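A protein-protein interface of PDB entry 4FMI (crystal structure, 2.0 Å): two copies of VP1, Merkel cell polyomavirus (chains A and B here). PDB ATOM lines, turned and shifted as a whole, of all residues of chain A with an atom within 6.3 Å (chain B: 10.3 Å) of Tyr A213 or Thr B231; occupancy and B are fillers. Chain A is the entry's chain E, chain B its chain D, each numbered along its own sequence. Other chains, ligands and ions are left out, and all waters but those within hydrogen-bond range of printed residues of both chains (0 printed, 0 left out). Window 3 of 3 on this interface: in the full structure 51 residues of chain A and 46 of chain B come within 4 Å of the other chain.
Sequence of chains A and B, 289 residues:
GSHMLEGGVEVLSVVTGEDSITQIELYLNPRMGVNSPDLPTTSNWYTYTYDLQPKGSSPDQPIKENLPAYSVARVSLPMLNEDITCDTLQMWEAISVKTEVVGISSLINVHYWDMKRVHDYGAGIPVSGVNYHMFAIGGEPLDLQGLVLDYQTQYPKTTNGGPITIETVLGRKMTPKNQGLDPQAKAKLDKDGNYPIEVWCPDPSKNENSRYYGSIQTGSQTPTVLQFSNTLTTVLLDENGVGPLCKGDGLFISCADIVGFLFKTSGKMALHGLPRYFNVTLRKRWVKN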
ATOM      1  N   VAL A  97     -18.571  -0.749  -1.659  1.00  0.00           N
ATOM      2  CA  VAL A  97     -18.234  -1.520  -2.862  1.00  0.00           C
ATOM      3  C   VAL A  97     -17.000  -2.377  -2.631  1.00  0.00           C
ATOM      4  O   VAL A  97     -16.022  -1.922  -2.014  1.00  0.00           O
ATOM      5  CB  VAL A  97     -18.047  -0.610  -4.126  1.00  0.00           C
ATOM      6  CG1 VAL A  97     -16.973   0.476  -3.896  1.00  0.00           C
ATOM      7  CG2 VAL A  97     -17.727  -1.444  -5.376  1.00  0.00           C
ATOM      8  N   HIS A 133      -5.372   4.216 -13.093  1.00  0.00           N
ATOM      9  CA  HIS A 133      -6.423   3.394 -12.506  1.00  0.00           C
ATOM     10  C   HIS A 133      -7.411   4.265 -11.782  1.00  0.00           C
ATOM     11  O   HIS A 133      -7.024   5.077 -10.950  1.00  0.00           O
ATOM     12  CB  HIS A 133      -5.839   2.355 -11.536  1.00  0.00           C
ATOM     13  CG  HIS A 133      -4.847   1.443 -12.178  1.00  0.00           C
ATOM     14  ND1 HIS A 133      -5.213   0.282 -12.821  1.00  0.00           N
ATOM     15  CD2 HIS A 133      -3.505   1.552 -12.325  1.00  0.00           C
ATOM     16  CE1 HIS A 133      -4.137  -0.298 -13.321  1.00  0.00           C
ATOM     17  NE2 HIS A 133      -3.088   0.455 -13.037  1.00  0.00           N
ATOM     18  N   MET A 134      -8.688   4.103 -12.115  1.00  0.00           N
ATOM     19  CA  MET A 134      -9.741   4.792 -11.393  1.00  0.00           C
ATOM     20  C   MET A 134     -11.031   4.002 -11.471  1.00  0.00           C
ATOM     21  O   MET A 134     -11.239   3.241 -12.413  1.00  0.00           O
ATOM     22  CB  MET A 134      -9.932   6.245 -11.894  1.00  0.00           C
ATOM     23  CG  MET A 134     -10.653   6.394 -13.219  1.00  0.00           C
ATOM     24  SD  MET A 134     -12.456   6.358 -13.059  1.00  0.00           S
ATOM     25  CE  MET A 134     -12.771   7.999 -12.440  1.00  0.00           C
ATOM     26  N   PHE A 135     -11.863   4.170 -10.447  1.00  0.00           N
ATOM     27  CA  PHE A 135     -13.228   3.666 -10.451  1.00  0.00           C
ATOM     28  C   PHE A 135     -14.129   4.687  -9.763  1.00  0.00           C
ATOM     29  O   PHE A 135     -13.652   5.550  -9.024  1.00  0.00           O
ATOM     30  CB  PHE A 135     -13.328   2.268  -9.808  1.00  0.00           C
ATOM     31  CG  PHE A 135     -13.242   2.257  -8.294  1.00  0.00           C
ATOM     32  CD1 PHE A 135     -12.004   2.196  -7.649  1.00  0.00           C
ATOM     33  CD2 PHE A 135     -14.407   2.260  -7.515  1.00  0.00           C
ATOM     34  CE1 PHE A 135     -11.927   2.161  -6.250  1.00  0.00           C
ATOM     35  CE2 PHE A 135     -14.344   2.231  -6.113  1.00  0.00           C
ATOM     36  CZ  PHE A 135     -13.098   2.178  -5.477  1.00  0.00           C
ATOM     37  N   ALA A 136     -15.427   4.592 -10.030  1.00  0.00           N
ATOM     38  CA  ALA A 136     -16.400   5.547  -9.527  1.00  0.00           C
ATOM     39  C   ALA A 136     -17.758   4.885  -9.371  1.00  0.00           C
ATOM     40  O   ALA A 136     -18.169   4.103 -10.229  1.00  0.00           O
ATOM     41  CB  ALA A 136     -16.504   6.766 -10.469  1.00  0.00           C
ATOM     42  N   ILE A 137     -18.438   5.216  -8.270  1.00  0.00           N
ATOM     43  CA  ILE A 137     -19.800   4.775  -7.987  1.00  0.00           C
ATOM     44  C   ILE A 137     -20.639   6.030  -7.712  1.00  0.00           C
ATOM     45  O   ILE A 137     -20.234   6.894  -6.919  1.00  0.00           O
ATOM     46  CB  ILE A 137     -19.864   3.807  -6.755  1.00  0.00           C
ATOM     47  CG1 ILE A 137     -18.772   2.718  -6.802  1.00  0.00           C
ATOM     48  CG2 ILE A 137     -21.265   3.208  -6.597  1.00  0.00           C
ATOM     49  CD1 ILE A 137     -18.819   1.735  -7.995  1.00  0.00           C
ATOM     50  N   SER A 210     -21.476  11.236  -6.388  1.00  0.00           N
ATOM     51  CA  SER A 210     -20.587  10.162  -6.831  1.00  0.00           C
ATOM     52  C   SER A 210     -19.340  10.089  -5.957  1.00  0.00           C
ATOM     53  O   SER A 210     -18.867  11.117  -5.447  1.00  0.00           O
ATOM     54  CB  SER A 210     -20.121  10.404  -8.274  1.00  0.00           C
ATOM     55  OG  SER A 210     -21.132  10.117  -9.213  1.00  0.00           O
ATOM     56  N   ARG A 211     -18.787   8.885  -5.814  1.00  0.00           N
ATOM     57  CA  ARG A 211     -17.467   8.724  -5.199  1.00  0.00           C
ATOM     58  C   ARG A 211     -16.499   8.140  -6.234  1.00  0.00           C
ATOM     59  O   ARG A 211     -16.772   7.104  -6.831  1.00  0.00           O
ATOM     60  CB  ARG A 211     -17.515   7.824  -3.950  1.00  0.00           C
ATOM     61  CG  ARG A 211     -18.667   8.094  -2.958  1.00  0.00           C
ATOM     62  CD  ARG A 211     -18.569   9.440  -2.218  1.00  0.00           C
ATOM     63  NE  ARG A 211     -19.699   9.603  -1.301  1.00  0.00           N
ATOM     64  CZ  ARG A 211     -20.789  10.326  -1.549  1.00  0.00           C
ATOM     65  NH1 ARG A 211     -20.912  11.019  -2.677  1.00  0.00           N
ATOM     66  NH2 ARG A 211     -21.754  10.371  -0.652  1.00  0.00           N
ATOM     67  N   TYR A 212     -15.369   8.812  -6.436  1.00  0.00           N
ATOM     68  CA  TYR A 212     -14.361   8.335  -7.363  1.00  0.00           C
ATOM     69  C   TYR A 212     -12.974   8.313  -6.715  1.00  0.00           C
ATOM     70  O   TYR A 212     -12.691   9.099  -5.809  1.00  0.00           O
ATOM     71  CB  TYR A 212     -14.384   9.152  -8.674  1.00  0.00           C
ATOM     72  CG  TYR A 212     -14.002  10.607  -8.548  1.00  0.00           C
ATOM     73  CD1 TYR A 212     -12.660  10.985  -8.515  1.00  0.00           C
ATOM     74  CD2 TYR A 212     -14.975  11.609  -8.478  1.00  0.00           C
ATOM     75  CE1 TYR A 212     -12.283  12.305  -8.406  1.00  0.00           C
ATOM     76  CE2 TYR A 212     -14.603  12.959  -8.382  1.00  0.00           C
ATOM     77  CZ  TYR A 212     -13.252  13.290  -8.345  1.00  0.00           C
ATOM     78  OH  TYR A 212     -12.846  14.602  -8.249  1.00  0.00           O
ATOM     79  N   TYR A 213     -12.145   7.375  -7.175  1.00  0.00           N
ATOM     80  CA  TYR A 213     -10.803   7.117  -6.647  1.00  0.00           C
ATOM     81  C   TYR A 213      -9.930   6.721  -7.837  1.00  0.00           C
ATOM     82  O   TYR A 213     -10.306   5.844  -8.626  1.00  0.00           O
ATOM     83  CB  TYR A 213     -10.816   5.939  -5.646  1.00  0.00           C
ATOM     84  CG  TYR A 213     -12.002   5.930  -4.693  1.00  0.00           C
ATOM     85  CD1 TYR A 213     -11.865   6.338  -3.366  1.00  0.00           C
ATOM     86  CD2 TYR A 213     -13.263   5.512  -5.126  1.00  0.00           C
ATOM     87  CE1 TYR A 213     -12.965   6.328  -2.492  1.00  0.00           C
ATOM     88  CE2 TYR A 213     -14.362   5.507  -4.272  1.00  0.00           C
ATOM     89  CZ  TYR A 213     -14.212   5.914  -2.961  1.00  0.00           C
ATOM     90  OH  TYR A 213     -15.320   5.896  -2.131  1.00  0.00           O
ATOM     91  N   GLY A 214      -8.770   7.346  -7.966  1.00  0.00           N
ATOM     92  CA  GLY A 214      -7.887   7.047  -9.081  1.00  0.00           C
ATOM     93  C   GLY A 214      -6.441   7.431  -8.834  1.00  0.00           C
ATOM     94  O   GLY A 214      -6.109   8.022  -7.802  1.00  0.00           O
ATOM     95  N   SER A 215      -5.578   7.076  -9.784  1.00  0.00           N
ATOM     96  CA  SER A 215      -4.169   7.439  -9.716  1.00  0.00           C
ATOM     97  C   SER A 215      -3.569   7.289 -11.100  1.00  0.00           C
ATOM     98  O   SER A 215      -4.212   6.735 -12.005  1.00  0.00           O
ATOM     99  CB  SER A 215      -3.427   6.530  -8.725  1.00  0.00           C
ATOM    100  OG  SER A 215      -3.432   5.176  -9.159  1.00  0.00           O
ATOM    101  N   THR A 234     -14.560  -0.827   0.083  1.00  0.00           N
ATOM    102  CA  THR A 234     -14.512   0.627   0.115  1.00  0.00           C
ATOM    103  C   THR A 234     -15.866   1.152   0.590  1.00  0.00           C
ATOM    104  O   THR A 234     -16.906   0.817   0.020  1.00  0.00           O
ATOM    105  CB  THR A 234     -14.138   1.200  -1.266  1.00  0.00           C
ATOM    106  OG1 THR A 234     -12.804   0.790  -1.591  1.00  0.00           O
ATOM    107  CG2 THR A 234     -14.217   2.736  -1.280  1.00  0.00           C
ATOM    108  N   VAL A 235     -15.841   1.952   1.656  1.00  0.00           N
ATOM    109  CA  VAL A 235     -17.044   2.550   2.215  1.00  0.00           C
ATOM    110  C   VAL A 235     -17.373   3.781   1.373  1.00  0.00           C
ATOM    111  O   VAL A 235     -16.501   4.611   1.115  1.00  0.00           O
ATOM    112  CB  VAL A 235     -16.862   2.916   3.718  1.00  0.00           C
ATOM    113  CG1 VAL A 235     -18.085   3.665   4.259  1.00  0.00           C
ATOM    114  CG2 VAL A 235     -16.609   1.648   4.562  1.00  0.00           C
ATOM    115  N   LEU A 236     -18.625   3.877   0.938  1.00  0.00           N
ATOM    116  CA  LEU A 236     -19.053   4.949   0.028  1.00  0.00           C
ATOM    117  C   LEU A 236     -19.792   6.126   0.700  1.00  0.00           C
ATOM    118  O   LEU A 236     -20.192   7.084   0.027  1.00  0.00           O
ATOM    119  CB  LEU A 236     -19.912   4.363  -1.095  1.00  0.00           C
ATOM    120  CG  LEU A 236     -19.236   3.417  -2.098  1.00  0.00           C
ATOM    121  CD1 LEU A 236     -20.298   2.794  -2.986  1.00  0.00           C
ATOM    122  CD2 LEU A 236     -18.166   4.128  -2.931  1.00  0.00           C
ATOM    123  N   LEU A 237     -19.963   6.047   2.020  1.00  0.00           N
ATOM    124  CA  LEU A 237     -20.647   7.085   2.795  1.00  0.00           C
ATOM    125  C   LEU A 237     -19.793   8.344   2.904  1.00  0.00           C
ATOM    126  O   LEU A 237     -18.576   8.265   3.120  1.00  0.00           O
ATOM    127  CB  LEU A 237     -21.006   6.563   4.197  1.00  0.00           C
ATOM    128  CG  LEU A 237     -21.808   5.254   4.276  1.00  0.00           C
ATOM    129  CD1 LEU A 237     -21.982   4.791   5.713  1.00  0.00           C
ATOM    130  CD2 LEU A 237     -23.166   5.394   3.592  1.00  0.00           C
ATOM    131  N   VAL B  97     -10.470  21.530   3.938  1.00  0.00           N
ATOM    132  CA  VAL B  97     -10.386  21.730   2.488  1.00  0.00           C
ATOM    133  C   VAL B  97     -10.342  20.402   1.730  1.00  0.00           C
ATOM    134  O   VAL B  97      -9.673  19.444   2.145  1.00  0.00           O
ATOM    135  CB  VAL B  97      -9.181  22.647   2.095  1.00  0.00           C
ATOM    136  CG1 VAL B  97      -7.847  22.061   2.580  1.00  0.00           C
ATOM    137  CG2 VAL B  97      -9.150  22.916   0.587  1.00  0.00           C
ATOM    138  N   LYS B  98     -11.118  20.342   0.652  1.00  0.00           N
ATOM    139  CA  LYS B  98     -10.968  19.303  -0.348  1.00  0.00           C
ATOM    140  C   LYS B  98     -10.205  19.956  -1.485  1.00  0.00           C
ATOM    141  O   LYS B  98     -10.645  20.973  -2.021  1.00  0.00           O
ATOM    142  CB  LYS B  98     -12.326  18.825  -0.855  1.00  0.00           C
ATOM    143  CG  LYS B  98     -13.066  17.863   0.047  1.00  0.00           C
ATOM    144  CD  LYS B  98     -14.263  17.312  -0.720  1.00  0.00           C
ATOM    145  CE  LYS B  98     -14.887  16.130  -0.036  1.00  0.00           C
ATOM    146  NZ  LYS B  98     -16.085  15.686  -0.800  1.00  0.00           N
ATOM    147  N   THR B  99      -9.061  19.393  -1.840  1.00  0.00           N
ATOM    148  CA  THR B  99      -8.263  19.941  -2.923  1.00  0.00           C
ATOM    149  C   THR B  99      -7.827  18.805  -3.825  1.00  0.00           C
ATOM    150  O   THR B  99      -7.675  17.661  -3.371  1.00  0.00           O
ATOM    151  CB  THR B  99      -7.044  20.765  -2.402  1.00  0.00           C
ATOM    152  OG1 THR B  99      -6.337  21.349  -3.509  1.00  0.00           O
ATOM    153  CG2 THR B  99      -6.104  19.897  -1.570  1.00  0.00           C
ATOM    154  N   GLU B 100      -7.654  19.107  -5.105  1.00  0.00           N
ATOM    155  CA  GLU B 100      -7.362  18.074  -6.080  1.00  0.00           C
ATOM    156  C   GLU B 100      -6.624  18.651  -7.271  1.00  0.00           C
ATOM    157  O   GLU B 100      -6.953  19.748  -7.743  1.00  0.00           O
ATOM    158  CB  GLU B 100      -8.673  17.397  -6.531  1.00  0.00           C
ATOM    159  CG  GLU B 100      -8.527  16.394  -7.683  1.00  0.00           C
ATOM    160  CD  GLU B 100      -9.789  15.567  -7.895  1.00  0.00           C
ATOM    161  OE1 GLU B 100     -10.298  14.987  -6.919  1.00  0.00           O
ATOM    162  OE2 GLU B 100     -10.276  15.498  -9.039  1.00  0.00           O
ATOM    163  N   ILE B 104      -5.060  15.249 -14.427  1.00  0.00           N
ATOM    164  CA  ILE B 104      -4.007  14.242 -14.233  1.00  0.00           C
ATOM    165  C   ILE B 104      -4.029  13.243 -15.388  1.00  0.00           C
ATOM    166  O   ILE B 104      -2.984  12.879 -15.918  1.00  0.00           O
ATOM    167  CB  ILE B 104      -4.126  13.548 -12.830  1.00  0.00           C
ATOM    168  CG1 ILE B 104      -3.660  14.510 -11.720  1.00  0.00           C
ATOM    169  CG2 ILE B 104      -3.337  12.237 -12.769  1.00  0.00           C
ATOM    170  CD1 ILE B 104      -3.908  14.016 -10.278  1.00  0.00           C
ATOM    171  N   LEU B 226       0.547  10.317  -9.006  1.00  0.00           N
ATOM    172  CA  LEU B 226      -0.414  11.220  -8.373  1.00  0.00           C
ATOM    173  C   LEU B 226      -1.740  10.495  -8.161  1.00  0.00           C
ATOM    174  O   LEU B 226      -2.104   9.634  -8.948  1.00  0.00           O
ATOM    175  CB  LEU B 226      -0.646  12.464  -9.250  1.00  0.00           C
ATOM    176  CG  LEU B 226       0.600  13.262  -9.661  1.00  0.00           C
ATOM    177  CD1 LEU B 226       0.284  14.211 -10.792  1.00  0.00           C
ATOM    178  CD2 LEU B 226       1.189  14.001  -8.480  1.00  0.00           C
ATOM    179  N   GLN B 227      -2.454  10.851  -7.100  1.00  0.00           N
ATOM    180  CA  GLN B 227      -3.768  10.278  -6.845  1.00  0.00           C
ATOM    181  C   GLN B 227      -4.838  11.356  -6.929  1.00  0.00           C
ATOM    182  O   GLN B 227      -4.543  12.547  -6.818  1.00  0.00           O
ATOM    183  CB  GLN B 227      -3.812   9.584  -5.481  1.00  0.00           C
ATOM    184  CG  GLN B 227      -2.799   8.445  -5.313  1.00  0.00           C
ATOM    185  CD  GLN B 227      -1.430   8.960  -4.890  1.00  0.00           C
ATOM    186  OE1 GLN B 227      -1.328   9.942  -4.146  1.00  0.00           O
ATOM    187  NE2 GLN B 227      -0.370   8.314  -5.372  1.00  0.00           N
ATOM    188  N   PHE B 228      -6.077  10.929  -7.137  1.00  0.00           N
ATOM    189  CA  PHE B 228      -7.203  11.848  -7.147  1.00  0.00           C
ATOM    190  C   PHE B 228      -8.451  11.133  -6.659  1.00  0.00           C
ATOM    191  O   PHE B 228      -8.744  10.016  -7.079  1.00  0.00           O
ATOM    192  CB  PHE B 228      -7.409  12.498  -8.535  1.00  0.00           C
ATOM    193  CG  PHE B 228      -7.542  11.511  -9.664  1.00  0.00           C
ATOM    194  CD1 PHE B 228      -6.404  10.986 -10.288  1.00  0.00           C
ATOM    195  CD2 PHE B 228      -8.802  11.103 -10.104  1.00  0.00           C
ATOM    196  CE1 PHE B 228      -6.518  10.063 -11.327  1.00  0.00           C
ATOM    197  CE2 PHE B 228      -8.934  10.168 -11.142  1.00  0.00           C
ATOM    198  CZ  PHE B 228      -7.791   9.648 -11.753  1.00  0.00           C
ATOM    199  N   SER B 229      -9.170  11.785  -5.752  1.00  0.00           N
ATOM    200  CA  SER B 229     -10.405  11.250  -5.191  1.00  0.00           C
ATOM    201  C   SER B 229     -11.175  12.394  -4.561  1.00  0.00           C
ATOM    202  O   SER B 229     -10.567  13.271  -3.940  1.00  0.00           O
ATOM    203  CB  SER B 229     -10.101  10.190  -4.128  1.00  0.00           C
ATOM    204  OG  SER B 229     -11.296   9.745  -3.498  1.00  0.00           O
ATOM    205  N   ASN B 230     -12.502  12.385  -4.711  1.00  0.00           N
ATOM    206  CA  ASN B 230     -13.343  13.404  -4.071  1.00  0.00           C
ATOM    207  C   ASN B 230     -13.785  13.040  -2.652  1.00  0.00           C
ATOM    208  O   ASN B 230     -14.734  13.610  -2.122  1.00  0.00           O
ATOM    209  CB  ASN B 230     -14.558  13.739  -4.942  1.00  0.00           C
ATOM    210  CG  ASN B 230     -15.530  12.577  -5.076  1.00  0.00           C
ATOM    211  OD1 ASN B 230     -15.164  11.408  -4.904  1.00  0.00           O
ATOM    212  ND2 ASN B 230     -16.774  12.895  -5.392  1.00  0.00           N
ATOM    213  N   THR B 231     -13.101  12.076  -2.050  1.00  0.00           N
ATOM    214  CA  THR B 231     -13.445  11.591  -0.726  1.00  0.00           C
ATOM    215  C   THR B 231     -12.400  12.046   0.285  1.00  0.00           C
ATOM    216  O   THR B 231     -12.507  11.730   1.467  1.00  0.00           O
ATOM    217  CB  THR B 231     -13.525  10.041  -0.688  1.00  0.00           C
ATOM    218  OG1 THR B 231     -12.213   9.488  -0.843  1.00  0.00           O
ATOM    219  CG2 THR B 231     -14.446   9.491  -1.786  1.00  0.00           C
ATOM    220  N   LEU B 232     -11.384  12.766  -0.185  1.00  0.00           N
ATOM    221  CA  LEU B 232     -10.247  13.145   0.654  1.00  0.00           C
ATOM    222  C   LEU B 232     -10.336  14.589   1.161  1.00  0.00           C
ATOM    223  O   LEU B 232     -10.445  15.522   0.367  1.00  0.00           O
ATOM    224  CB  LEU B 232      -8.923  12.916  -0.094  1.00  0.00           C
ATOM    225  CG  LEU B 232      -8.496  11.448  -0.308  1.00  0.00           C
ATOM    226  CD1 LEU B 232      -7.289  11.336  -1.232  1.00  0.00           C
ATOM    227  CD2 LEU B 232      -8.232  10.725   1.023  1.00  0.00           C
ATOM    228  N   THR B 233     -10.275  14.750   2.484  1.00  0.00           N
ATOM    229  CA  THR B 233     -10.410  16.042   3.149  1.00  0.00           C
ATOM    230  C   THR B 233      -9.165  16.332   3.979  1.00  0.00           C
ATOM    231  O   THR B 233      -8.634  15.438   4.643  1.00  0.00           O
ATOM    232  CB  THR B 233     -11.643  16.043   4.077  1.00  0.00           C
ATOM    233  OG1 THR B 233     -12.824  15.863   3.289  1.00  0.00           O
ATOM    234  CG2 THR B 233     -11.762  17.349   4.864  1.00  0.00           C
ATOM    235  N   THR B 234      -8.692  17.573   3.929  1.00  0.00           N
ATOM    236  CA  THR B 234      -7.619  18.012   4.819  1.00  0.00           C
ATOM    237  C   THR B 234      -8.166  18.927   5.926  1.00  0.00           C
ATOM    238  O   THR B 234      -8.713  20.001   5.648  1.00  0.00           O
ATOM    239  CB  THR B 234      -6.492  18.696   4.037  1.00  0.00           C
ATOM    240  OG1 THR B 234      -5.929  17.754   3.117  1.00  0.00           O
ATOM    241  CG2 THR B 234      -5.386  19.169   4.966  1.00  0.00           C
ATOM    242  N   VAL B 235      -8.025  18.479   7.173  1.00  0.00           N
ATOM    243  CA  VAL B 235      -8.409  19.259   8.344  1.00  0.00           C
ATOM    244  C   VAL B 235      -7.377  20.368   8.564  1.00  0.00           C
ATOM    245  O   VAL B 235      -6.176  20.096   8.579  1.00  0.00           O
ATOM    246  CB  VAL B 235      -8.555  18.349   9.597  1.00  0.00           C
ATOM    247  CG1 VAL B 235      -8.761  19.175  10.876  1.00  0.00           C
ATOM    248  CG2 VAL B 235      -9.714  17.367   9.409  1.00  0.00           C
ATOM    249  N   TYR B 277      -7.882  22.424  -7.887  1.00  0.00           N
ATOM    250  CA  TYR B 277      -9.203  22.777  -7.411  1.00  0.00           C
ATOM    251  C   TYR B 277      -9.197  22.811  -5.888  1.00  0.00           C
ATOM    252  O   TYR B 277      -8.492  22.027  -5.241  1.00  0.00           O
ATOM    253  CB  TYR B 277     -10.241  21.767  -7.938  1.00  0.00           C
ATOM    254  CG  TYR B 277     -11.606  21.858  -7.275  1.00  0.00           C
ATOM    255  CD1 TYR B 277     -12.543  22.812  -7.673  1.00  0.00           C
ATOM    256  CD2 TYR B 277     -11.951  20.991  -6.244  1.00  0.00           C
ATOM    257  CE1 TYR B 277     -13.786  22.902  -7.054  1.00  0.00           C
ATOM    258  CE2 TYR B 277     -13.193  21.065  -5.623  1.00  0.00           C
ATOM    259  CZ  TYR B 277     -14.101  22.016  -6.028  1.00  0.00           C
ATOM    260  OH  TYR B 277     -15.325  22.068  -5.408  1.00  0.00           O
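O of Phe B228 lies within hydrogen-bond range of N of Gly A214, 2.8 Å away. The side-chain hydroxyl of Tyr A212 sits at hydrogen-bond distance from the side-chain carboxylate of Glu B100 (2.8 Å). OD1 of Asn B230 sits at hydrogen-bond distance from N of Tyr A212, at 3.0 Å. ND2 of Asn B230 lies within hydrogen-bond range of O of Ser A210 (2.7 Å). The backbone carbonyl oxygen (O) of Tyr A212 sits at hydrogen-bond distance from the side-chain hydroxyl (OG) of Ser B229, at 2.8 Å.
The backbone NH of Tyr B277 sits at hydrogen-bond distance from the backbone carbonyl oxygen of Glu B100 (2.8 Å). The backbone NH (N) of Phe A135 sits at hydrogen-bond distance from the backbone carbonyl oxygen (O) of Tyr A213, at 2.9 Å. O of His A133 is in hydrogen-bond range of N of Ser A215 (2.7 Å). The side-chain amino group of Lys B98 lies within hydrogen-bond range of the backbone carbonyl oxygen of Asn B230 (2.8 Å). The backbone carbonyl oxygen (O) of Leu A236 sits at hydrogen-bond distance from the guanidinium group (NE) of Arg A211 (2.9 Å). The backbone carbonyl oxygen (O) of Ile A137 sits at hydrogen-bond distance from the backbone NH (N) of Arg A211 (2.7 Å).
Arg A211 touches Asn B230. Tyr A213 touches Phe B228. Tyr A213 touches Ser B229. Thr B231 touches Tyr A213 (CG2 to CE1, 3.6 Å). Gln B227 touches Gly A214 (CA to O, 3.4 Å). Leu B226 touches Ser A215. CB of Ser A215 touches CG of Gln B227 (3.96 Å). N of Ser A215 touches CE1 of Phe B228 (3.5 Å).
No residue of chain B comes within 4 Å of Met A134. Phe A135 touches none of the printed residues of chain B. Printed residues of chain B within 4 Å of Tyr A212: Glu B100, Ser B229 and Asn B230. Tyr A213 touches just these residues of chain B: Phe B228, Ser B229 and Thr B231. Of the printed residues of chain B, Gly A214 touches Gln B227 (3.4 Å) and Phe B228 (2.8 Å). Of the printed residues of chain B, Ser A215 touches Leu B226, Gln B227 and Phe B228. No residue of chain B comes within 4 Å of Leu A236. Lys B98 touches none of the printed residues of chain A. Of the printed residues of chain A, Gln B227 touches Gly A214 (3.4 Å) and Ser A215 (3.96 Å). Of the printed residues of chain A, Phe B228 touches Tyr A213, Gly A214 and Ser A215. Of the printed residues of chain A, Asn B230 touches Ser A210 (2.7 Å), Arg A211 (3.5 Å) and Tyr A212 (3.0 Å). Thr B231 touches just one residue of chain A: Tyr A213 (3.6 Å).
Hydrophobic or aromatic side chains of chain A within 4 Å of the printed part of chain B: Tyr A212 and Tyr A213. Of the 16 printed residues of chain B, 7 touch a printed residue of chain A. Among the printed residues, 13 pairs touch across the chains. Among the printed residues, no Asp or Glu carboxylate lies within 4 Å of a Lys or Arg side-chain nitrogen of the other chain.
Positions printed for both chains: 97, 234 and 235.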
